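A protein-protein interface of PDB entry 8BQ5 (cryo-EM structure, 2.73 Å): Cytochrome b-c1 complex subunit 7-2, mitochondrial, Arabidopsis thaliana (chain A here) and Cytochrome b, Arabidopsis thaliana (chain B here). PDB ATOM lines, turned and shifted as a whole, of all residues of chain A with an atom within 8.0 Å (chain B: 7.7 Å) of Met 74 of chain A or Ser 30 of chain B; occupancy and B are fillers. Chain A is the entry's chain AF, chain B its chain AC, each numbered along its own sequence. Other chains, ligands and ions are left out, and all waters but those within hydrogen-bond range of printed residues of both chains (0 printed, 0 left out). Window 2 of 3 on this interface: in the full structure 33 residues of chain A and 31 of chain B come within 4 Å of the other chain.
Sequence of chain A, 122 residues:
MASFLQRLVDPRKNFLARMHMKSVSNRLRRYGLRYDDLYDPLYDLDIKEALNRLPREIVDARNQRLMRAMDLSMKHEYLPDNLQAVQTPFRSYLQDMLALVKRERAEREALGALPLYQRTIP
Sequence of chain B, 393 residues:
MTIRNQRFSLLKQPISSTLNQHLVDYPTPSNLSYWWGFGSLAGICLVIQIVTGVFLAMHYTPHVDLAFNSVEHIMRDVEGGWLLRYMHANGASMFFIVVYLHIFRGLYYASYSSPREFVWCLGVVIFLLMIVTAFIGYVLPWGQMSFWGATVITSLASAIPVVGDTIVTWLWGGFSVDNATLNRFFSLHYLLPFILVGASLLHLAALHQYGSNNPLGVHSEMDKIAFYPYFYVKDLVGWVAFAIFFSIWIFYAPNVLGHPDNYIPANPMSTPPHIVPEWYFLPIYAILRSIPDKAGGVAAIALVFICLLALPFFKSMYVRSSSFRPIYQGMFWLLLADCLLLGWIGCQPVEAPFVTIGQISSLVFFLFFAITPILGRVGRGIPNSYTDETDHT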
ATOM      1  N   TYR A  31     -35.326   7.312  10.701  1.00  0.00           N
ATOM      2  CA  TYR A  31     -35.463   6.431   9.552  1.00  0.00           C
ATOM      3  C   TYR A  31     -36.863   6.438   8.957  1.00  0.00           C
ATOM      4  O   TYR A  31     -37.096   5.761   7.951  1.00  0.00           O
ATOM      5  CB  TYR A  31     -35.079   5.002   9.943  1.00  0.00           C
ATOM      6  CG  TYR A  31     -33.592   4.798  10.071  1.00  0.00           C
ATOM      7  CD1 TYR A  31     -32.777   4.790   8.950  1.00  0.00           C
ATOM      8  CD2 TYR A  31     -33.001   4.632  11.315  1.00  0.00           C
ATOM      9  CE1 TYR A  31     -31.417   4.610   9.063  1.00  0.00           C
ATOM     10  CE2 TYR A  31     -31.642   4.453  11.437  1.00  0.00           C
ATOM     11  CZ  TYR A  31     -30.855   4.441  10.308  1.00  0.00           C
ATOM     12  OH  TYR A  31     -29.497   4.262  10.424  1.00  0.00           O
ATOM     13  N   MET A  67     -38.636   0.107   2.728  1.00  0.00           N
ATOM     14  CA  MET A  67     -37.714   0.379   1.631  1.00  0.00           C
ATOM     15  C   MET A  67     -37.026   1.725   1.807  1.00  0.00           C
ATOM     16  O   MET A  67     -35.823   1.854   1.554  1.00  0.00           O
ATOM     17  CB  MET A  67     -38.454   0.327   0.295  1.00  0.00           C
ATOM     18  CG  MET A  67     -37.583   0.689  -0.890  1.00  0.00           C
ATOM     19  SD  MET A  67     -38.122  -0.056  -2.434  1.00  0.00           S
ATOM     20  CE  MET A  67     -36.613   0.036  -3.396  1.00  0.00           C
ATOM     21  N   ARG A  68     -37.777   2.742   2.235  1.00  0.00           N
ATOM     22  CA  ARG A  68     -37.180   4.051   2.475  1.00  0.00           C
ATOM     23  C   ARG A  68     -36.136   3.985   3.582  1.00  0.00           C
ATOM     24  O   ARG A  68     -35.052   4.566   3.459  1.00  0.00           O
ATOM     25  CB  ARG A  68     -38.271   5.065   2.820  1.00  0.00           C
ATOM     26  CG  ARG A  68     -37.755   6.434   3.217  1.00  0.00           C
ATOM     27  CD  ARG A  68     -38.898   7.420   3.390  1.00  0.00           C
ATOM     28  NE  ARG A  68     -39.683   7.153   4.589  1.00  0.00           N
ATOM     29  CZ  ARG A  68     -40.706   7.891   4.994  1.00  0.00           C
ATOM     30  NH1 ARG A  68     -41.092   8.964   4.323  1.00  0.00           N
ATOM     31  NH2 ARG A  68     -41.358   7.546   6.100  1.00  0.00           N
ATOM     32  N   ALA A  69     -36.445   3.278   4.672  1.00  0.00           N
ATOM     33  CA  ALA A  69     -35.497   3.163   5.774  1.00  0.00           C
ATOM     34  C   ALA A  69     -34.247   2.401   5.356  1.00  0.00           C
ATOM     35  O   ALA A  69     -33.128   2.774   5.732  1.00  0.00           O
ATOM     36  CB  ALA A  69     -36.161   2.480   6.967  1.00  0.00           C
ATOM     37  N   MET A  70     -34.415   1.323   4.590  1.00  0.00           N
ATOM     38  CA  MET A  70     -33.262   0.556   4.131  1.00  0.00           C
ATOM     39  C   MET A  70     -32.394   1.380   3.191  1.00  0.00           C
ATOM     40  O   MET A  70     -31.164   1.260   3.203  1.00  0.00           O
ATOM     41  CB  MET A  70     -33.728  -0.731   3.452  1.00  0.00           C
ATOM     42  CG  MET A  70     -33.854  -1.909   4.398  1.00  0.00           C
ATOM     43  SD  MET A  70     -33.969  -3.481   3.528  1.00  0.00           S
ATOM     44  CE  MET A  70     -32.259  -3.747   3.077  1.00  0.00           C
ATOM     45  N   ASP A  71     -33.020   2.215   2.359  1.00  0.00           N
ATOM     46  CA  ASP A  71     -32.259   3.100   1.486  1.00  0.00           C
ATOM     47  C   ASP A  71     -31.464   4.120   2.292  1.00  0.00           C
ATOM     48  O   ASP A  71     -30.303   4.405   1.975  1.00  0.00           O
ATOM     49  CB  ASP A  71     -33.201   3.800   0.508  1.00  0.00           C
ATOM     50  CG  ASP A  71     -32.491   4.810  -0.365  1.00  0.00           C
ATOM     51  OD1 ASP A  71     -31.557   4.414  -1.092  1.00  0.00           O
ATOM     52  OD2 ASP A  71     -32.867   6.000  -0.327  1.00  0.00           O
ATOM     53  N   LEU A  72     -32.073   4.687   3.336  1.00  0.00           N
ATOM     54  CA  LEU A  72     -31.358   5.629   4.191  1.00  0.00           C
ATOM     55  C   LEU A  72     -30.221   4.943   4.938  1.00  0.00           C
ATOM     56  O   LEU A  72     -29.130   5.507   5.076  1.00  0.00           O
ATOM     57  CB  LEU A  72     -32.323   6.285   5.178  1.00  0.00           C
ATOM     58  CG  LEU A  72     -33.346   7.255   4.592  1.00  0.00           C
ATOM     59  CD1 LEU A  72     -34.491   7.468   5.565  1.00  0.00           C
ATOM     60  CD2 LEU A  72     -32.685   8.576   4.242  1.00  0.00           C
ATOM     61  N   SER A  73     -30.462   3.726   5.429  1.00  0.00           N
ATOM     62  CA  SER A  73     -29.417   2.978   6.121  1.00  0.00           C
ATOM     63  C   SER A  73     -28.236   2.697   5.200  1.00  0.00           C
ATOM     64  O   SER A  73     -27.077   2.795   5.618  1.00  0.00           O
ATOM     65  CB  SER A  73     -29.988   1.673   6.674  1.00  0.00           C
ATOM     66  OG  SER A  73     -29.185   1.165   7.721  1.00  0.00           O
ATOM     67  N   MET A  74     -28.513   2.340   3.945  1.00  0.00           N
ATOM     68  CA  MET A  74     -27.439   2.077   2.994  1.00  0.00           C
ATOM     69  C   MET A  74     -26.624   3.334   2.717  1.00  0.00           C
ATOM     70  O   MET A  74     -25.392   3.277   2.621  1.00  0.00           O
ATOM     71  CB  MET A  74     -28.019   1.515   1.696  1.00  0.00           C
ATOM     72  CG  MET A  74     -26.981   1.204   0.635  1.00  0.00           C
ATOM     73  SD  MET A  74     -27.089   2.286  -0.803  1.00  0.00           S
ATOM     74  CE  MET A  74     -28.808   2.083  -1.259  1.00  0.00           C
ATOM     75  N   LYS A  75     -27.292   4.480   2.593  1.00  0.00           N
ATOM     76  CA  LYS A  75     -26.634   5.735   2.258  1.00  0.00           C
ATOM     77  C   LYS A  75     -25.990   6.420   3.457  1.00  0.00           C
ATOM     78  O   LYS A  75     -25.315   7.438   3.269  1.00  0.00           O
ATOM     79  CB  LYS A  75     -27.638   6.690   1.608  1.00  0.00           C
ATOM     80  CG  LYS A  75     -28.027   6.311   0.194  1.00  0.00           C
ATOM     81  CD  LYS A  75     -29.292   7.031  -0.234  1.00  0.00           C
ATOM     82  CE  LYS A  75     -29.538   6.872  -1.722  1.00  0.00           C
ATOM     83  NZ  LYS A  75     -30.901   7.326  -2.108  1.00  0.00           N
ATOM     84  N   HIS A  76     -26.187   5.900   4.670  1.00  0.00           N
ATOM     85  CA  HIS A  76     -25.626   6.482   5.891  1.00  0.00           C
ATOM     86  C   HIS A  76     -26.163   7.899   6.117  1.00  0.00           C
ATOM     87  O   HIS A  76     -25.468   8.792   6.602  1.00  0.00           O
ATOM     88  CB  HIS A  76     -24.091   6.451   5.854  1.00  0.00           C
ATOM     89  CG  HIS A  76     -23.433   6.943   7.106  1.00  0.00           C
ATOM     90  ND1 HIS A  76     -23.455   6.233   8.287  1.00  0.00           N
ATOM     91  CD2 HIS A  76     -22.722   8.067   7.357  1.00  0.00           C
ATOM     92  CE1 HIS A  76     -22.795   6.905   9.215  1.00  0.00           C
ATOM     93  NE2 HIS A  76     -22.340   8.021   8.675  1.00  0.00           N
ATOM     94  N   GLU A  77     -27.427   8.103   5.759  1.00  0.00           N
ATOM     95  CA  GLU A  77     -28.086   9.376   6.002  1.00  0.00           C
ATOM     96  C   GLU A  77     -29.402   9.130   6.721  1.00  0.00           C
ATOM     97  O   GLU A  77     -29.876   7.996   6.827  1.00  0.00           O
ATOM     98  CB  GLU A  77     -28.321  10.158   4.701  1.00  0.00           C
ATOM     99  CG  GLU A  77     -29.153   9.428   3.666  1.00  0.00           C
ATOM    100  CD  GLU A  77     -29.139  10.127   2.322  1.00  0.00           C
ATOM    101  OE1 GLU A  77     -28.037  10.408   1.809  1.00  0.00           O
ATOM    102  OE2 GLU A  77     -30.230  10.394   1.775  1.00  0.00           O
ATOM    103  N   PRO B  27     -29.671 -13.006  -3.203  1.00  0.00           N
ATOM    104  CA  PRO B  27     -30.248 -11.751  -2.693  1.00  0.00           C
ATOM    105  C   PRO B  27     -29.720 -11.349  -1.308  1.00  0.00           C
ATOM    106  O   PRO B  27     -29.888 -12.115  -0.386  1.00  0.00           O
ATOM    107  CB  PRO B  27     -31.748 -12.067  -2.635  1.00  0.00           C
ATOM    108  CG  PRO B  27     -31.938 -13.166  -3.645  1.00  0.00           C
ATOM    109  CD  PRO B  27     -30.697 -14.011  -3.485  1.00  0.00           C
ATOM    110  N   THR B  28     -29.129 -10.158  -1.189  1.00  0.00           N
ATOM    111  CA  THR B  28     -28.529  -9.701   0.049  1.00  0.00           C
ATOM    112  C   THR B  28     -29.064  -8.318   0.395  1.00  0.00           C
ATOM    113  O   THR B  28     -29.208  -7.473  -0.495  1.00  0.00           O
ATOM    114  CB  THR B  28     -26.997  -9.652  -0.084  1.00  0.00           C
ATOM    115  OG1 THR B  28     -26.533 -10.859  -0.702  1.00  0.00           O
ATOM    116  CG2 THR B  28     -26.335  -9.509   1.270  1.00  0.00           C
ATOM    117  N   PRO B  29     -29.383  -8.062   1.664  1.00  0.00           N
ATOM    118  CA  PRO B  29     -29.855  -6.724   2.049  1.00  0.00           C
ATOM    119  C   PRO B  29     -28.843  -5.654   1.670  1.00  0.00           C
ATOM    120  O   PRO B  29     -27.643  -5.799   1.902  1.00  0.00           O
ATOM    121  CB  PRO B  29     -30.018  -6.834   3.569  1.00  0.00           C
ATOM    122  CG  PRO B  29     -30.290  -8.276   3.798  1.00  0.00           C
ATOM    123  CD  PRO B  29     -29.447  -9.007   2.792  1.00  0.00           C
ATOM    124  N   SER B  30     -29.344  -4.561   1.092  1.00  0.00           N
ATOM    125  CA  SER B  30     -28.459  -3.547   0.531  1.00  0.00           C
ATOM    126  C   SER B  30     -27.782  -2.695   1.596  1.00  0.00           C
ATOM    127  O   SER B  30     -26.807  -2.004   1.286  1.00  0.00           O
ATOM    128  CB  SER B  30     -29.235  -2.650  -0.433  1.00  0.00           C
ATOM    129  OG  SER B  30     -30.164  -1.838   0.263  1.00  0.00           O
ATOM    130  N   ASN B  31     -28.263  -2.730   2.838  1.00  0.00           N
ATOM    131  CA  ASN B  31     -27.745  -1.868   3.891  1.00  0.00           C
ATOM    132  C   ASN B  31     -26.800  -2.597   4.841  1.00  0.00           C
ATOM    133  O   ASN B  31     -26.579  -2.127   5.963  1.00  0.00           O
ATOM    134  CB  ASN B  31     -28.900  -1.238   4.671  1.00  0.00           C
ATOM    135  CG  ASN B  31     -29.657  -2.246   5.510  1.00  0.00           C
ATOM    136  OD1 ASN B  31     -29.819  -3.399   5.117  1.00  0.00           O
ATOM    137  ND2 ASN B  31     -30.125  -1.814   6.674  1.00  0.00           N
ATOM    138  N   LEU B  32     -26.235  -3.727   4.419  1.00  0.00           N
ATOM    139  CA  LEU B  32     -25.274  -4.433   5.257  1.00  0.00           C
ATOM    140  C   LEU B  32     -24.013  -3.598   5.431  1.00  0.00           C
ATOM    141  O   LEU B  32     -23.473  -3.057   4.463  1.00  0.00           O
ATOM    142  CB  LEU B  32     -24.925  -5.789   4.648  1.00  0.00           C
ATOM    143  CG  LEU B  32     -25.994  -6.880   4.683  1.00  0.00           C
ATOM    144  CD1 LEU B  32     -25.355  -8.237   4.469  1.00  0.00           C
ATOM    145  CD2 LEU B  32     -26.754  -6.846   5.992  1.00  0.00           C
ATOM    146  N   SER B  33     -23.542  -3.503   6.669  1.00  0.00           N
ATOM    147  CA  SER B  33     -22.359  -2.723   6.982  1.00  0.00           C
ATOM    148  C   SER B  33     -21.108  -3.589   6.854  1.00  0.00           C
ATOM    149  O   SER B  33     -21.155  -4.737   6.406  1.00  0.00           O
ATOM    150  CB  SER B  33     -22.478  -2.121   8.381  1.00  0.00           C
ATOM    151  OG  SER B  33     -22.109  -3.062   9.371  1.00  0.00           O
ATOM    152  N   SER B 212     -29.616 -13.142   5.222  1.00  0.00           N
ATOM    153  CA  SER B 212     -28.894 -12.508   6.311  1.00  0.00           C
ATOM    154  C   SER B 212     -29.740 -11.431   6.982  1.00  0.00           C
ATOM    155  O   SER B 212     -30.620 -10.823   6.368  1.00  0.00           O
ATOM    156  CB  SER B 212     -27.587 -11.902   5.801  1.00  0.00           C
ATOM    157  OG  SER B 212     -27.788 -10.586   5.325  1.00  0.00           O
ATOM    158  N   ASN B 214     -29.991  -7.683   8.901  1.00  0.00           N
ATOM    159  CA  ASN B 214     -29.502  -6.379   8.484  1.00  0.00           C
ATOM    160  C   ASN B 214     -29.394  -5.472   9.701  1.00  0.00           C
ATOM    161  O   ASN B 214     -29.972  -5.767  10.753  1.00  0.00           O
ATOM    162  CB  ASN B 214     -30.411  -5.754   7.414  1.00  0.00           C
ATOM    163  CG  ASN B 214     -31.798  -5.449   7.928  1.00  0.00           C
ATOM    164  OD1 ASN B 214     -32.043  -4.384   8.491  1.00  0.00           O
ATOM    165  ND2 ASN B 214     -32.721  -6.381   7.728  1.00  0.00           N
ATOM    166  N   PRO B 215     -28.634  -4.375   9.600  1.00  0.00           N
ATOM    167  CA  PRO B 215     -28.434  -3.511  10.778  1.00  0.00           C
ATOM    168  C   PRO B 215     -29.716  -2.963  11.380  1.00  0.00           C
ATOM    169  O   PRO B 215     -29.744  -2.682  12.584  1.00  0.00           O
ATOM    170  CB  PRO B 215     -27.548  -2.383  10.235  1.00  0.00           C
ATOM    171  CG  PRO B 215     -26.819  -2.987   9.108  1.00  0.00           C
ATOM    172  CD  PRO B 215     -27.721  -4.018   8.498  1.00  0.00           C
ATOM    173  N   LEU B 216     -30.772  -2.781  10.587  1.00  0.00           N
ATOM    174  CA  LEU B 216     -32.031  -2.289  11.134  1.00  0.00           C
ATOM    175  C   LEU B 216     -32.864  -3.391  11.775  1.00  0.00           C
ATOM    176  O   LEU B 216     -33.806  -3.085  12.514  1.00  0.00           O
ATOM    177  CB  LEU B 216     -32.845  -1.598  10.040  1.00  0.00           C
ATOM    178  CG  LEU B 216     -32.276  -0.291   9.484  1.00  0.00           C
ATOM    179  CD1 LEU B 216     -33.129   0.208   8.334  1.00  0.00           C
ATOM    180  CD2 LEU B 216     -32.167   0.765  10.571  1.00  0.00           C
ATOM    181  N   SER B 220     -36.329  -7.334   5.051  1.00  0.00           N
ATOM    182  CA  SER B 220     -35.470  -6.710   4.053  1.00  0.00           C
ATOM    183  C   SER B 220     -35.766  -7.167   2.632  1.00  0.00           C
ATOM    184  O   SER B 220     -34.968  -6.889   1.730  1.00  0.00           O
ATOM    185  CB  SER B 220     -33.998  -6.977   4.380  1.00  0.00           C
ATOM    186  OG  SER B 220     -33.767  -8.358   4.590  1.00  0.00           O
ATOM    187  N   MET B 222     -37.553  -6.102   0.398  1.00  0.00           N
ATOM    188  CA  MET B 222     -37.914  -5.032  -0.575  1.00  0.00           C
ATOM    189  C   MET B 222     -36.672  -4.346  -1.151  1.00  0.00           C
ATOM    190  O   MET B 222     -36.829  -3.620  -2.147  1.00  0.00           O
ATOM    191  CB  MET B 222     -38.787  -3.973   0.106  1.00  0.00           C
ATOM    192  CG  MET B 222     -38.057  -3.157   1.154  1.00  0.00           C
ATOM    193  SD  MET B 222     -39.160  -2.181   2.203  1.00  0.00           S
ATOM    194  CE  MET B 222     -39.537  -3.359   3.499  1.00  0.00           C
ATOM    195  N   ASP B 223     -35.490  -4.567  -0.572  1.00  0.00           N
ATOM    196  CA  ASP B 223     -34.295  -3.850  -1.015  1.00  0.00           C
ATOM    197  C   ASP B 223     -33.078  -4.770  -1.035  1.00  0.00           C
ATOM    198  O   ASP B 223     -32.006  -4.429  -0.534  1.00  0.00           O
ATOM    199  CB  ASP B 223     -34.039  -2.632  -0.130  1.00  0.00           C
ATOM    200  CG  ASP B 223     -33.249  -1.552  -0.841  1.00  0.00           C
ATOM    201  OD1 ASP B 223     -32.893  -1.751  -2.020  1.00  0.00           O
ATOM    202  OD2 ASP B 223     -32.984  -0.502  -0.219  1.00  0.00           O
ATOM    203  N   LYS B 224     -33.224  -5.950  -1.626  1.00  0.00           N
ATOM    204  CA  LYS B 224     -32.117  -6.888  -1.733  1.00  0.00           C
ATOM    205  C   LYS B 224     -31.396  -6.718  -3.065  1.00  0.00           C
ATOM    206  O   LYS B 224     -32.005  -6.397  -4.088  1.00  0.00           O
ATOM    207  CB  LYS B 224     -32.599  -8.331  -1.582  1.00  0.00           C
ATOM    208  CG  LYS B 224     -33.314  -8.596  -0.275  1.00  0.00           C
ATOM    209  CD  LYS B 224     -33.201 -10.044   0.149  1.00  0.00           C
ATOM    210  CE  LYS B 224     -32.893 -10.146   1.630  1.00  0.00           C
ATOM    211  NZ  LYS B 224     -33.771 -11.136   2.310  1.00  0.00           N
ATOM    212  N   ILE B 225     -30.081  -6.940  -3.038  1.00  0.00           N
ATOM    213  CA  ILE B 225     -29.242  -6.868  -4.225  1.00  0.00           C
ATOM    214  C   ILE B 225     -28.389  -8.128  -4.291  1.00  0.00           C
ATOM    215  O   ILE B 225     -28.243  -8.862  -3.312  1.00  0.00           O
ATOM    216  CB  ILE B 225     -28.347  -5.611  -4.245  1.00  0.00           C
ATOM    217  CG1 ILE B 225     -27.698  -5.390  -2.879  1.00  0.00           C
ATOM    218  CG2 ILE B 225     -29.153  -4.391  -4.650  1.00  0.00           C
ATOM    219  CD1 ILE B 225     -26.516  -4.451  -2.915  1.00  0.00           C
ATOM    220  N   TYR B 230     -21.527  -6.405  -5.537  1.00  0.00           N
ATOM    221  CA  TYR B 230     -21.595  -5.344  -4.535  1.00  0.00           C
ATOM    222  C   TYR B 230     -20.973  -5.771  -3.214  1.00  0.00           C
ATOM    223  O   TYR B 230     -20.167  -5.039  -2.632  1.00  0.00           O
ATOM    224  CB  TYR B 230     -23.043  -4.903  -4.343  1.00  0.00           C
ATOM    225  CG  TYR B 230     -23.656  -4.405  -5.621  1.00  0.00           C
ATOM    226  CD1 TYR B 230     -23.408  -3.115  -6.061  1.00  0.00           C
ATOM    227  CD2 TYR B 230     -24.463  -5.223  -6.396  1.00  0.00           C
ATOM    228  CE1 TYR B 230     -23.949  -2.649  -7.228  1.00  0.00           C
ATOM    229  CE2 TYR B 230     -25.014  -4.764  -7.570  1.00  0.00           C
ATOM    230  CZ  TYR B 230     -24.751  -3.473  -7.978  1.00  0.00           C
ATOM    231  OH  TYR B 230     -25.287  -2.991  -9.145  1.00  0.00           O
ATOM    232  N   PHE B 231     -21.334  -6.949  -2.717  1.00  0.00           N
ATOM    233  CA  PHE B 231     -20.743  -7.399  -1.467  1.00  0.00           C
ATOM    234  C   PHE B 231     -19.475  -8.205  -1.684  1.00  0.00           C
ATOM    235  O   PHE B 231     -18.783  -8.521  -0.712  1.00  0.00           O
ATOM    236  CB  PHE B 231     -21.772  -8.185  -0.663  1.00  0.00           C
ATOM    237  CG  PHE B 231     -22.884  -7.331  -0.155  1.00  0.00           C
ATOM    238  CD1 PHE B 231     -22.672  -6.469   0.904  1.00  0.00           C
ATOM    239  CD2 PHE B 231     -24.124  -7.345  -0.767  1.00  0.00           C
ATOM    240  CE1 PHE B 231     -23.682  -5.660   1.365  1.00  0.00           C
ATOM    241  CE2 PHE B 231     -25.138  -6.538  -0.309  1.00  0.00           C
ATOM    242  CZ  PHE B 231     -24.916  -5.693   0.758  1.00  0.00           C
ATOM    243  N   LYS B 234     -17.072  -5.202  -1.481  1.00  0.00           N
ATOM    244  CA  LYS B 234     -17.053  -4.731  -0.071  1.00  0.00           C
ATOM    245  C   LYS B 234     -16.264  -5.743   0.762  1.00  0.00           C
ATOM    246  O   LYS B 234     -15.523  -5.308   1.656  1.00  0.00           O
ATOM    247  CB  LYS B 234     -18.480  -4.514   0.441  1.00  0.00           C
ATOM    248  CG  LYS B 234     -18.588  -3.791   1.774  1.00  0.00           C
ATOM    249  CD  LYS B 234     -19.972  -3.273   2.080  1.00  0.00           C
ATOM    250  CE  LYS B 234     -20.016  -2.496   3.377  1.00  0.00           C
ATOM    251  NZ  LYS B 234     -21.244  -1.678   3.491  1.00  0.00           N
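The side-chain hydroxyl of Ser 73 of chain A is in hydrogen-bond range of the side-chain amide nitrogen of Asn 31 of chain B (3.3 Å). SD of Met 222 of chain B sits at hydrogen-bond distance from N of Met 67 of chain A (2.4 Å).
The backbone NH (N) of Ser 30 of chain B is in hydrogen-bond range of the backbone carbonyl oxygen (O) of Asp 223 of chain B. The side-chain amide oxygen (OD1) of Asn 214 of chain B lies within hydrogen-bond range of the backbone NH (N) of Leu 216 of chain B (2.9 Å). OD2 of Asp 71 of chain A lies within salt-bridge range of NZ of Lys 75 of chain A (3.0 Å).
Among the printed residues, pairs that only touch across the chains: Met 70 of chain A with Asn 31 of chain B (3.2 Å), Met 74 of chain A with Ser 30 of chain B (3.3 Å), Met 70 of chain A with Ser 220 of chain B (3.6 Å), Met 70 of chain A with Ser 30 of chain B (3.6 Å), Ala 69 of chain A with Leu 216 of chain B (3.7 Å), Met 74 of chain A with Asn 31 of chain B (3.7 Å), Met 70 of chain A with Asp 223 of chain B (3.7 Å), Asp 71 of chain A with Asp 223 of chain B (3.7 Å), Tyr 31 of chain A with Leu 216 of chain B (3.8 Å), Ser 73 of chain A with Leu 216 of chain B (3.8 Å) and Met 70 of chain A with Pro 29 of chain B (3.8 Å).
Printed residues of chain B within 4 Å of Ala 69 of chain A: Leu 216 (3.7 Å). Printed residues of chain B within 4 Å of Asp 71 of chain A: Asp 223. Ser 30 of chain B touches two residues of chain A. Printed residues of chain A within 4 Å of Asn 31 of chain B: Met 70, Ser 73 and Met 74. Ile 225 of chain B touches none of the printed residues of chain A. Lys 234 of chain B touches none of the printed residues of chain A. The nearest residue of chain B that does not touch Met 74 of chain A is Asp 223 of chain B (5.0 Å). The nearest residue of chain A that does not touch Ser 30 of chain B is Asp 71 of chain A (5.4 Å). The nearest printed residue of chain B that does not touch Ala 69 of chain A is Asn 31 of chain B (5.6 Å).
Printed residues of chain B that touch a printed residue of chain A: Pro 29, Ser 30, Asn 31, Leu 216, Ser 220, Met 222 and Asp 223. Hydrophobic or aromatic side chains of chain A within 4 Å of the printed part of chain B: Tyr 31, Met 67, Met 70 and Met 74. Among the printed residues, 13 pairs touch across the chains. Among the printed residues, no Asp or Glu carboxylate lies within 4 Å of a Lys or Arg side-chain nitrogen of the other chain.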
